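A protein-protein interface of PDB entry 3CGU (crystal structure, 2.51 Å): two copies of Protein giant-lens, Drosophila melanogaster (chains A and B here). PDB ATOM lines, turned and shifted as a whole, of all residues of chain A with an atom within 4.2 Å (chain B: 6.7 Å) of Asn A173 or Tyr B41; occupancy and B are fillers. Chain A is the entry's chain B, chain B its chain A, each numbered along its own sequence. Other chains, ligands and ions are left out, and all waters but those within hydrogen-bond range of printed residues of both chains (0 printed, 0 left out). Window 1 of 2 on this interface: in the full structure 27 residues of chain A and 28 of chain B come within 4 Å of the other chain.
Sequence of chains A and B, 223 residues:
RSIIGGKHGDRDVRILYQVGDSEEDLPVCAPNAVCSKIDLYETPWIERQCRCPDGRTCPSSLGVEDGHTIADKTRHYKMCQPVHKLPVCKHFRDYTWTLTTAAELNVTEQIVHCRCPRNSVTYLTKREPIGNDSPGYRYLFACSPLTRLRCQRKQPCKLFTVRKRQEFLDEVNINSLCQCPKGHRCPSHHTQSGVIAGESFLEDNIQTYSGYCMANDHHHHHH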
ATOM      1  N   LYS A  73      24.467  14.261 -24.849  1.00  0.00           N
ATOM      2  CA  LYS A  73      25.702  13.994 -24.147  1.00  0.00           C
ATOM      3  C   LYS A  73      26.847  14.826 -24.718  1.00  0.00           C
ATOM      4  O   LYS A  73      26.834  16.052 -24.675  1.00  0.00           O
ATOM      5  CB  LYS A  73      26.059  12.509 -24.234  1.00  0.00           C
ATOM      6  CG  LYS A  73      25.225  11.611 -23.342  1.00  0.00           C
ATOM      7  CD  LYS A  73      25.909  10.245 -23.175  1.00  0.00           C
ATOM      8  CE  LYS A  73      25.843   9.426 -24.474  1.00  0.00           C
ATOM      9  NZ  LYS A  73      24.491   8.789 -24.601  1.00  0.00           N
ATOM     10  N   LEU A 159      21.674  -0.931 -18.497  1.00  0.00           N
ATOM     11  CA  LEU A 159      22.473  -0.863 -19.724  1.00  0.00           C
ATOM     12  C   LEU A 159      23.851  -0.233 -19.486  1.00  0.00           C
ATOM     13  O   LEU A 159      23.955   0.822 -18.872  1.00  0.00           O
ATOM     14  CB  LEU A 159      21.736  -0.081 -20.793  1.00  0.00           C
ATOM     15  CG  LEU A 159      22.399  -0.242 -22.158  1.00  0.00           C
ATOM     16  CD1 LEU A 159      21.749  -1.399 -22.943  1.00  0.00           C
ATOM     17  CD2 LEU A 159      22.303   1.057 -22.938  1.00  0.00           C
ATOM     18  N   PHE A 160      24.899  -0.899 -19.966  1.00  0.00           N
ATOM     19  CA  PHE A 160      26.273  -0.428 -19.816  1.00  0.00           C
ATOM     20  C   PHE A 160      26.825  -0.067 -21.180  1.00  0.00           C
ATOM     21  O   PHE A 160      26.786  -0.884 -22.096  1.00  0.00           O
ATOM     22  CB  PHE A 160      27.168  -1.516 -19.223  1.00  0.00           C
ATOM     23  CG  PHE A 160      26.748  -1.987 -17.855  1.00  0.00           C
ATOM     24  CD1 PHE A 160      27.174  -1.329 -16.724  1.00  0.00           C
ATOM     25  CD2 PHE A 160      25.947  -3.107 -17.712  1.00  0.00           C
ATOM     26  CE1 PHE A 160      26.793  -1.757 -15.476  1.00  0.00           C
ATOM     27  CE2 PHE A 160      25.564  -3.545 -16.471  1.00  0.00           C
ATOM     28  CZ  PHE A 160      25.980  -2.862 -15.349  1.00  0.00           C
ATOM     29  N   THR A 161      27.336   1.149 -21.320  1.00  0.00           N
ATOM     30  CA  THR A 161      27.972   1.569 -22.564  1.00  0.00           C
ATOM     31  C   THR A 161      29.436   1.927 -22.309  1.00  0.00           C
ATOM     32  O   THR A 161      29.740   2.950 -21.705  1.00  0.00           O
ATOM     33  CB  THR A 161      27.255   2.778 -23.184  1.00  0.00           C
ATOM     34  OG1 THR A 161      25.872   2.462 -23.361  1.00  0.00           O
ATOM     35  CG2 THR A 161      27.858   3.142 -24.540  1.00  0.00           C
ATOM     36  N   GLU A 171      35.291   5.092 -20.538  1.00  0.00           N
ATOM     37  CA  GLU A 171      34.156   5.770 -19.951  1.00  0.00           C
ATOM     38  C   GLU A 171      32.953   4.836 -20.001  1.00  0.00           C
ATOM     39  O   GLU A 171      32.548   4.407 -21.075  1.00  0.00           O
ATOM     40  CB  GLU A 171      33.865   7.052 -20.723  1.00  0.00           C
ATOM     41  CG  GLU A 171      32.560   7.719 -20.325  1.00  0.00           C
ATOM     42  CD  GLU A 171      32.189   8.870 -21.261  1.00  0.00           C
ATOM     43  OE1 GLU A 171      31.000   8.950 -21.666  1.00  0.00           O
ATOM     44  OE2 GLU A 171      33.090   9.683 -21.601  1.00  0.00           O
ATOM     45  N   VAL A 172      32.393   4.521 -18.840  1.00  0.00           N
ATOM     46  CA  VAL A 172      31.277   3.598 -18.742  1.00  0.00           C
ATOM     47  C   VAL A 172      30.010   4.383 -18.430  1.00  0.00           C
ATOM     48  O   VAL A 172      29.888   4.959 -17.374  1.00  0.00           O
ATOM     49  CB  VAL A 172      31.508   2.549 -17.592  1.00  0.00           C
ATOM     50  CG1 VAL A 172      30.348   1.630 -17.458  1.00  0.00           C
ATOM     51  CG2 VAL A 172      32.788   1.762 -17.802  1.00  0.00           C
ATOM     52  N   ASN A 173      29.062   4.412 -19.341  1.00  0.00           N
ATOM     53  CA  ASN A 173      27.773   4.976 -19.016  1.00  0.00           C
ATOM     54  C   ASN A 173      26.814   3.885 -18.583  1.00  0.00           C
ATOM     55  O   ASN A 173      26.577   2.927 -19.320  1.00  0.00           O
ATOM     56  CB  ASN A 173      27.196   5.714 -20.215  1.00  0.00           C
ATOM     57  CG  ASN A 173      27.594   7.163 -20.239  1.00  0.00           C
ATOM     58  OD1 ASN A 173      26.752   8.039 -20.117  1.00  0.00           O
ATOM     59  ND2 ASN A 173      28.886   7.425 -20.365  1.00  0.00           N
ATOM     60  N   ILE A 174      26.262   4.006 -17.390  1.00  0.00           N
ATOM     61  CA  ILE A 174      25.306   3.016 -16.963  1.00  0.00           C
ATOM     62  C   ILE A 174      23.898   3.585 -16.814  1.00  0.00           C
ATOM     63  O   ILE A 174      23.643   4.449 -15.968  1.00  0.00           O
ATOM     64  CB  ILE A 174      25.782   2.253 -15.704  1.00  0.00           C
ATOM     65  CG1 ILE A 174      24.583   1.739 -14.916  1.00  0.00           C
ATOM     66  CG2 ILE A 174      26.689   3.119 -14.860  1.00  0.00           C
ATOM     67  CD1 ILE A 174      25.003   0.831 -13.777  1.00  0.00           C
ATOM     68  N   ASN A 175      22.993   3.112 -17.670  1.00  0.00           N
ATOM     69  CA  ASN A 175      21.583   3.500 -17.614  1.00  0.00           C
ATOM     70  C   ASN A 175      20.715   2.558 -16.778  1.00  0.00           C
ATOM     71  O   ASN A 175      20.792   1.343 -16.925  1.00  0.00           O
ATOM     72  CB  ASN A 175      21.005   3.579 -19.025  1.00  0.00           C
ATOM     73  CG  ASN A 175      21.349   4.867 -19.717  1.00  0.00           C
ATOM     74  OD1 ASN A 175      21.983   4.872 -20.780  1.00  0.00           O
ATOM     75  ND2 ASN A 175      20.945   5.978 -19.112  1.00  0.00           N
ATOM     76  N   ILE B  38      32.547  26.543 -18.387  1.00  0.00           N
ATOM     77  CA  ILE B  38      31.537  26.182 -19.369  1.00  0.00           C
ATOM     78  C   ILE B  38      31.299  24.685 -19.342  1.00  0.00           C
ATOM     79  O   ILE B  38      32.213  23.901 -19.580  1.00  0.00           O
ATOM     80  CB  ILE B  38      31.954  26.626 -20.790  1.00  0.00           C
ATOM     81  CG1 ILE B  38      32.187  28.135 -20.815  1.00  0.00           C
ATOM     82  CG2 ILE B  38      30.904  26.251 -21.797  1.00  0.00           C
ATOM     83  CD1 ILE B  38      32.549  28.672 -22.190  1.00  0.00           C
ATOM     84  N   ASP B  39      30.074  24.281 -19.031  1.00  0.00           N
ATOM     85  CA  ASP B  39      29.715  22.874 -19.132  1.00  0.00           C
ATOM     86  C   ASP B  39      28.961  22.621 -20.423  1.00  0.00           C
ATOM     87  O   ASP B  39      27.987  23.294 -20.716  1.00  0.00           O
ATOM     88  CB  ASP B  39      28.870  22.421 -17.947  1.00  0.00           C
ATOM     89  CG  ASP B  39      28.463  20.966 -18.062  1.00  0.00           C
ATOM     90  OD1 ASP B  39      27.570  20.643 -18.883  1.00  0.00           O
ATOM     91  OD2 ASP B  39      29.047  20.137 -17.331  1.00  0.00           O
ATOM     92  N   LEU B  40      29.412  21.635 -21.185  1.00  0.00           N
ATOM     93  CA  LEU B  40      28.851  21.362 -22.499  1.00  0.00           C
ATOM     94  C   LEU B  40      28.223  19.971 -22.593  1.00  0.00           C
ATOM     95  O   LEU B  40      28.203  19.376 -23.669  1.00  0.00           O
ATOM     96  CB  LEU B  40      29.957  21.483 -23.542  1.00  0.00           C
ATOM     97  CG  LEU B  40      30.540  22.880 -23.784  1.00  0.00           C
ATOM     98  CD1 LEU B  40      31.923  22.779 -24.412  1.00  0.00           C
ATOM     99  CD2 LEU B  40      29.613  23.686 -24.665  1.00  0.00           C
ATOM    100  N   TYR B  41      27.710  19.452 -21.478  1.00  0.00           N
ATOM    101  CA  TYR B  41      27.207  18.078 -21.452  1.00  0.00           C
ATOM    102  C   TYR B  41      25.851  17.910 -22.129  1.00  0.00           C
ATOM    103  O   TYR B  41      25.732  17.203 -23.120  1.00  0.00           O
ATOM    104  CB  TYR B  41      27.161  17.515 -20.026  1.00  0.00           C
ATOM    105  CG  TYR B  41      26.880  16.030 -19.983  1.00  0.00           C
ATOM    106  CD1 TYR B  41      25.618  15.550 -19.682  1.00  0.00           C
ATOM    107  CD2 TYR B  41      27.875  15.112 -20.277  1.00  0.00           C
ATOM    108  CE1 TYR B  41      25.357  14.191 -19.653  1.00  0.00           C
ATOM    109  CE2 TYR B  41      27.628  13.746 -20.252  1.00  0.00           C
ATOM    110  CZ  TYR B  41      26.367  13.286 -19.933  1.00  0.00           C
ATOM    111  OH  TYR B  41      26.117  11.921 -19.896  1.00  0.00           O
ATOM    112  N   GLU B  42      24.813  18.520 -21.586  1.00  0.00           N
ATOM    113  CA  GLU B  42      23.544  18.506 -22.298  1.00  0.00           C
ATOM    114  C   GLU B  42      23.348  19.886 -22.905  1.00  0.00           C
ATOM    115  O   GLU B  42      23.866  20.183 -23.983  1.00  0.00           O
ATOM    116  CB  GLU B  42      22.377  18.149 -21.371  1.00  0.00           C
ATOM    117  CG  GLU B  42      22.229  16.666 -21.064  1.00  0.00           C
ATOM    118  CD  GLU B  42      21.947  15.839 -22.312  1.00  0.00           C
ATOM    119  OE1 GLU B  42      20.766  15.441 -22.523  1.00  0.00           O
ATOM    120  OE2 GLU B  42      22.908  15.591 -23.090  1.00  0.00           O
ATOM    121  N   THR B  43      22.606  20.722 -22.182  1.00  0.00           N
ATOM    122  CA  THR B  43      22.424  22.126 -22.524  1.00  0.00           C
ATOM    123  C   THR B  43      23.611  22.923 -22.035  1.00  0.00           C
ATOM    124  O   THR B  43      23.829  23.011 -20.836  1.00  0.00           O
ATOM    125  CB  THR B  43      21.189  22.700 -21.826  1.00  0.00           C
ATOM    126  OG1 THR B  43      20.011  21.987 -22.271  1.00  0.00           O
ATOM    127  CG2 THR B  43      21.053  24.212 -22.124  1.00  0.00           C
ATOM    128  N   PRO B  44      24.367  23.534 -22.959  1.00  0.00           N
ATOM    129  CA  PRO B  44      25.581  24.253 -22.584  1.00  0.00           C
ATOM    130  C   PRO B  44      25.268  25.419 -21.643  1.00  0.00           C
ATOM    131  O   PRO B  44      24.358  26.199 -21.908  1.00  0.00           O
ATOM    132  CB  PRO B  44      26.086  24.802 -23.924  1.00  0.00           C
ATOM    133  CG  PRO B  44      25.397  24.002 -24.969  1.00  0.00           C
ATOM    134  CD  PRO B  44      24.090  23.625 -24.403  1.00  0.00           C
ATOM    135  N   TRP B  45      25.999  25.531 -20.544  1.00  0.00           N
ATOM    136  CA  TRP B  45      25.895  26.720 -19.716  1.00  0.00           C
ATOM    137  C   TRP B  45      27.248  27.231 -19.259  1.00  0.00           C
ATOM    138  O   TRP B  45      28.213  26.473 -19.152  1.00  0.00           O
ATOM    139  CB  TRP B  45      24.951  26.524 -18.521  1.00  0.00           C
ATOM    140  CG  TRP B  45      25.198  25.318 -17.646  1.00  0.00           C
ATOM    141  CD1 TRP B  45      24.496  24.147 -17.652  1.00  0.00           C
ATOM    142  CD2 TRP B  45      26.186  25.188 -16.613  1.00  0.00           C
ATOM    143  NE1 TRP B  45      24.992  23.289 -16.699  1.00  0.00           N
ATOM    144  CE2 TRP B  45      26.027  23.904 -16.044  1.00  0.00           C
ATOM    145  CE3 TRP B  45      27.194  26.029 -16.120  1.00  0.00           C
ATOM    146  CZ2 TRP B  45      26.837  23.437 -15.009  1.00  0.00           C
ATOM    147  CZ3 TRP B  45      28.001  25.563 -15.085  1.00  0.00           C
ATOM    148  CH2 TRP B  45      27.818  24.278 -14.545  1.00  0.00           C
ATOM    149  N   THR B  74      34.561  17.520 -20.469  1.00  0.00           N
ATOM    150  CA  THR B  74      33.226  17.944 -20.719  1.00  0.00           C
ATOM    151  C   THR B  74      33.083  19.409 -20.420  1.00  0.00           C
ATOM    152  O   THR B  74      32.014  19.963 -20.444  1.00  0.00           O
ATOM    153  CB  THR B  74      32.298  17.161 -19.815  1.00  0.00           C
ATOM    154  OG1 THR B  74      31.122  17.906 -19.562  1.00  0.00           O
ATOM    155  CG2 THR B  74      32.952  16.932 -18.510  1.00  0.00           C
ATOM    156  N   ARG B  75      34.199  20.036 -20.149  1.00  0.00           N
ATOM    157  CA  ARG B  75      34.221  21.375 -19.621  1.00  0.00           C
ATOM    158  C   ARG B  75      35.247  22.270 -20.295  1.00  0.00           C
ATOM    159  O   ARG B  75      36.246  21.789 -20.810  1.00  0.00           O
ATOM    160  CB  ARG B  75      34.512  21.296 -18.135  1.00  0.00           C
ATOM    161  CG  ARG B  75      33.321  20.818 -17.326  1.00  0.00           C
ATOM    162  CD  ARG B  75      33.633  20.853 -15.841  1.00  0.00           C
ATOM    163  NE  ARG B  75      32.490  21.312 -15.059  1.00  0.00           N
ATOM    164  CZ  ARG B  75      32.568  21.730 -13.794  1.00  0.00           C
ATOM    165  NH1 ARG B  75      33.740  21.747 -13.152  1.00  0.00           N
ATOM    166  NH2 ARG B  75      31.472  22.143 -13.171  1.00  0.00           N
ATOM    167  N   ARG B 165      25.128  11.721 -13.066  1.00  0.00           N
ATOM    168  CA  ARG B 165      24.616  12.638 -14.079  1.00  0.00           C
ATOM    169  C   ARG B 165      23.161  12.990 -13.853  1.00  0.00           C
ATOM    170  O   ARG B 165      22.750  14.127 -14.077  1.00  0.00           O
ATOM    171  CB  ARG B 165      24.781  12.050 -15.474  1.00  0.00           C
ATOM    172  CG  ARG B 165      26.205  12.070 -15.970  1.00  0.00           C
ATOM    173  CD  ARG B 165      26.680  13.481 -16.181  1.00  0.00           C
ATOM    174  NE  ARG B 165      28.027  13.519 -16.736  1.00  0.00           N
ATOM    175  CZ  ARG B 165      28.680  14.645 -17.024  1.00  0.00           C
ATOM    176  NH1 ARG B 165      28.103  15.821 -16.802  1.00  0.00           N
ATOM    177  NH2 ARG B 165      29.908  14.594 -17.529  1.00  0.00           N
ATOM    178  N   GLN B 166      22.372  12.003 -13.436  1.00  0.00           N
ATOM    179  CA  GLN B 166      20.992  12.260 -13.040  1.00  0.00           C
ATOM    180  C   GLN B 166      20.398  11.067 -12.314  1.00  0.00           C
ATOM    181  O   GLN B 166      21.108  10.092 -12.008  1.00  0.00           O
ATOM    182  CB  GLN B 166      20.129  12.633 -14.238  1.00  0.00           C
ATOM    183  CG  GLN B 166      20.277  11.709 -15.412  1.00  0.00           C
ATOM    184  CD  GLN B 166      19.195  11.951 -16.439  1.00  0.00           C
ATOM    185  OE1 GLN B 166      19.462  12.424 -17.546  1.00  0.00           O
ATOM    186  NE2 GLN B 166      17.953  11.645 -16.068  1.00  0.00           N
ATOM    187  N   LEU B 169      21.258   7.834 -14.346  1.00  0.00           N
ATOM    188  CA  LEU B 169      22.393   7.832 -15.243  1.00  0.00           C
ATOM    189  C   LEU B 169      23.649   8.143 -14.471  1.00  0.00           C
ATOM    190  O   LEU B 169      23.799   9.234 -13.924  1.00  0.00           O
ATOM    191  CB  LEU B 169      22.205   8.874 -16.340  1.00  0.00           C
ATOM    192  CG  LEU B 169      23.346   9.048 -17.346  1.00  0.00           C
ATOM    193  CD1 LEU B 169      23.662   7.725 -18.040  1.00  0.00           C
ATOM    194  CD2 LEU B 169      22.975  10.109 -18.376  1.00  0.00           C
ATOM    195  N   ASP B 170      24.555   7.173 -14.425  1.00  0.00           N
ATOM    196  CA  ASP B 170      25.865   7.356 -13.818  1.00  0.00           C
ATOM    197  C   ASP B 170      26.958   7.240 -14.872  1.00  0.00           C
ATOM    198  O   ASP B 170      26.874   6.444 -15.804  1.00  0.00           O
ATOM    199  CB  ASP B 170      26.097   6.312 -12.730  1.00  0.00           C
ATOM    200  CG  ASP B 170      24.927   6.200 -11.779  1.00  0.00           C
ATOM    201  OD1 ASP B 170      24.735   5.096 -11.205  1.00  0.00           O
ATOM    202  OD2 ASP B 170      24.188   7.209 -11.609  1.00  0.00           O
ATOM    203  N   GLU B 171      27.992   8.040 -14.717  1.00  0.00           N
ATOM    204  CA  GLU B 171      29.061   8.054 -15.676  1.00  0.00           C
ATOM    205  C   GLU B 171      30.313   7.779 -14.890  1.00  0.00           C
ATOM    206  O   GLU B 171      30.617   8.493 -13.940  1.00  0.00           O
ATOM    207  CB  GLU B 171      29.132   9.417 -16.371  1.00  0.00           C
ATOM    208  CG  GLU B 171      30.366   9.603 -17.243  1.00  0.00           C
ATOM    209  CD  GLU B 171      30.492  11.028 -17.797  1.00  0.00           C
ATOM    210  OE1 GLU B 171      31.592  11.633 -17.654  1.00  0.00           O
ATOM    211  OE2 GLU B 171      29.489  11.543 -18.360  1.00  0.00           O
ATOM    212  N   VAL B 172      31.022   6.723 -15.259  1.00  0.00           N
ATOM    213  CA  VAL B 172      32.214   6.319 -14.531  1.00  0.00           C
ATOM    214  C   VAL B 172      33.411   6.482 -15.444  1.00  0.00           C
ATOM    215  O   VAL B 172      33.542   5.775 -16.427  1.00  0.00           O
ATOM    216  CB  VAL B 172      32.127   4.825 -14.093  1.00  0.00           C
ATOM    217  CG1 VAL B 172      33.404   4.384 -13.432  1.00  0.00           C
ATOM    218  CG2 VAL B 172      30.932   4.593 -13.178  1.00  0.00           C
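Hydrophobic or aromatic side chains of chain A within 4 Å of the printed part of chain B: Val A172 and Ile A174. Printed residues of chain B that touch a printed residue of chain A: Leu B40, Tyr B41, Glu B42, Leu B169, Asp B170, Glu B171 and Val B172. Hydrophobic or aromatic side chains of chain B within 4 Å of the printed part of chain A: Tyr B41, Leu B169 and Val B172. Among the printed residues, 13 pairs touch across the chains.
Among the printed residues, pairs that only touch across the chains: Lys A73 with Leu B40 (3.7 Å), Glu A171 with Val B172 (3.6 Å), Val A172 with Asp B170 (3.7 Å), Val A172 with Glu B171 (3.6 Å), Asn A173 with Tyr B41 (3.9 Å), Asn A173 with Leu B169 (3.7 Å), Asn A173 with Asp B170 (3.6 Å), Ile A174 with Leu B169 (3.7 Å) and Asn A175 with Leu B169 (3.4 Å).
Glu A171 touches Val B172, and with the chains exchanged Val A172 touches Glu B171. Val B172 touches its own counterpart, Val A172. Positions printed for both chains: 171 and 172. Of the 13 pairs that touch across the chains among the printed residues, 3 have their exchanged pair printed and touching as well.
Tyr B41 touches two residues of chain A. Of the printed residues of chain A, Val B172 touches Glu A171 (3.6 Å) and Val A172 (3.0 Å). Printed residues of chain A within 4 Å of Asp B170: Val A172, Asn A173 and Ile A174. Thr B74 touches none of the printed residues of chain A. The nearest printed residue of chain A that does not touch Tyr B41 is Glu A171 (6.0 Å).
O of Leu A159 sits at hydrogen-bond distance from N of Asn A175, 2.8 Å away. The guanidinium group (NE) of Arg B165 lies within salt-bridge range of the side-chain carboxylate (OE2) of Glu B171. ND2 of Asn A173 sits at hydrogen-bond distance from OE1 of Glu A171, 2.9 Å away. The backbone carbonyl oxygen of Thr B74 sits at hydrogen-bond distance from the backbone NH of Leu B40, at 3.2 Å. OD1 of Asp B39 lies within hydrogen-bond range of N of Tyr B41, at 2.9 Å. N of Thr A161 lies within hydrogen-bond range of O of Asn A173 (2.8 Å).
The backbone carbonyl oxygen (O) of Lys A73 sits close to the backbone carbonyl oxygen (O) of Tyr B41 (2.2 Å). The backbone carbonyl oxygen of Asp B170 is in hydrogen-bond range of the backbone NH of Ile A174. The side-chain carboxylate of Glu B42 sits at hydrogen-bond distance from the backbone NH of Lys A73, 2.7 Å away. The backbone carbonyl oxygen (O) of Val B172 lies within hydrogen-bond range of the backbone NH (N) of Val A172.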
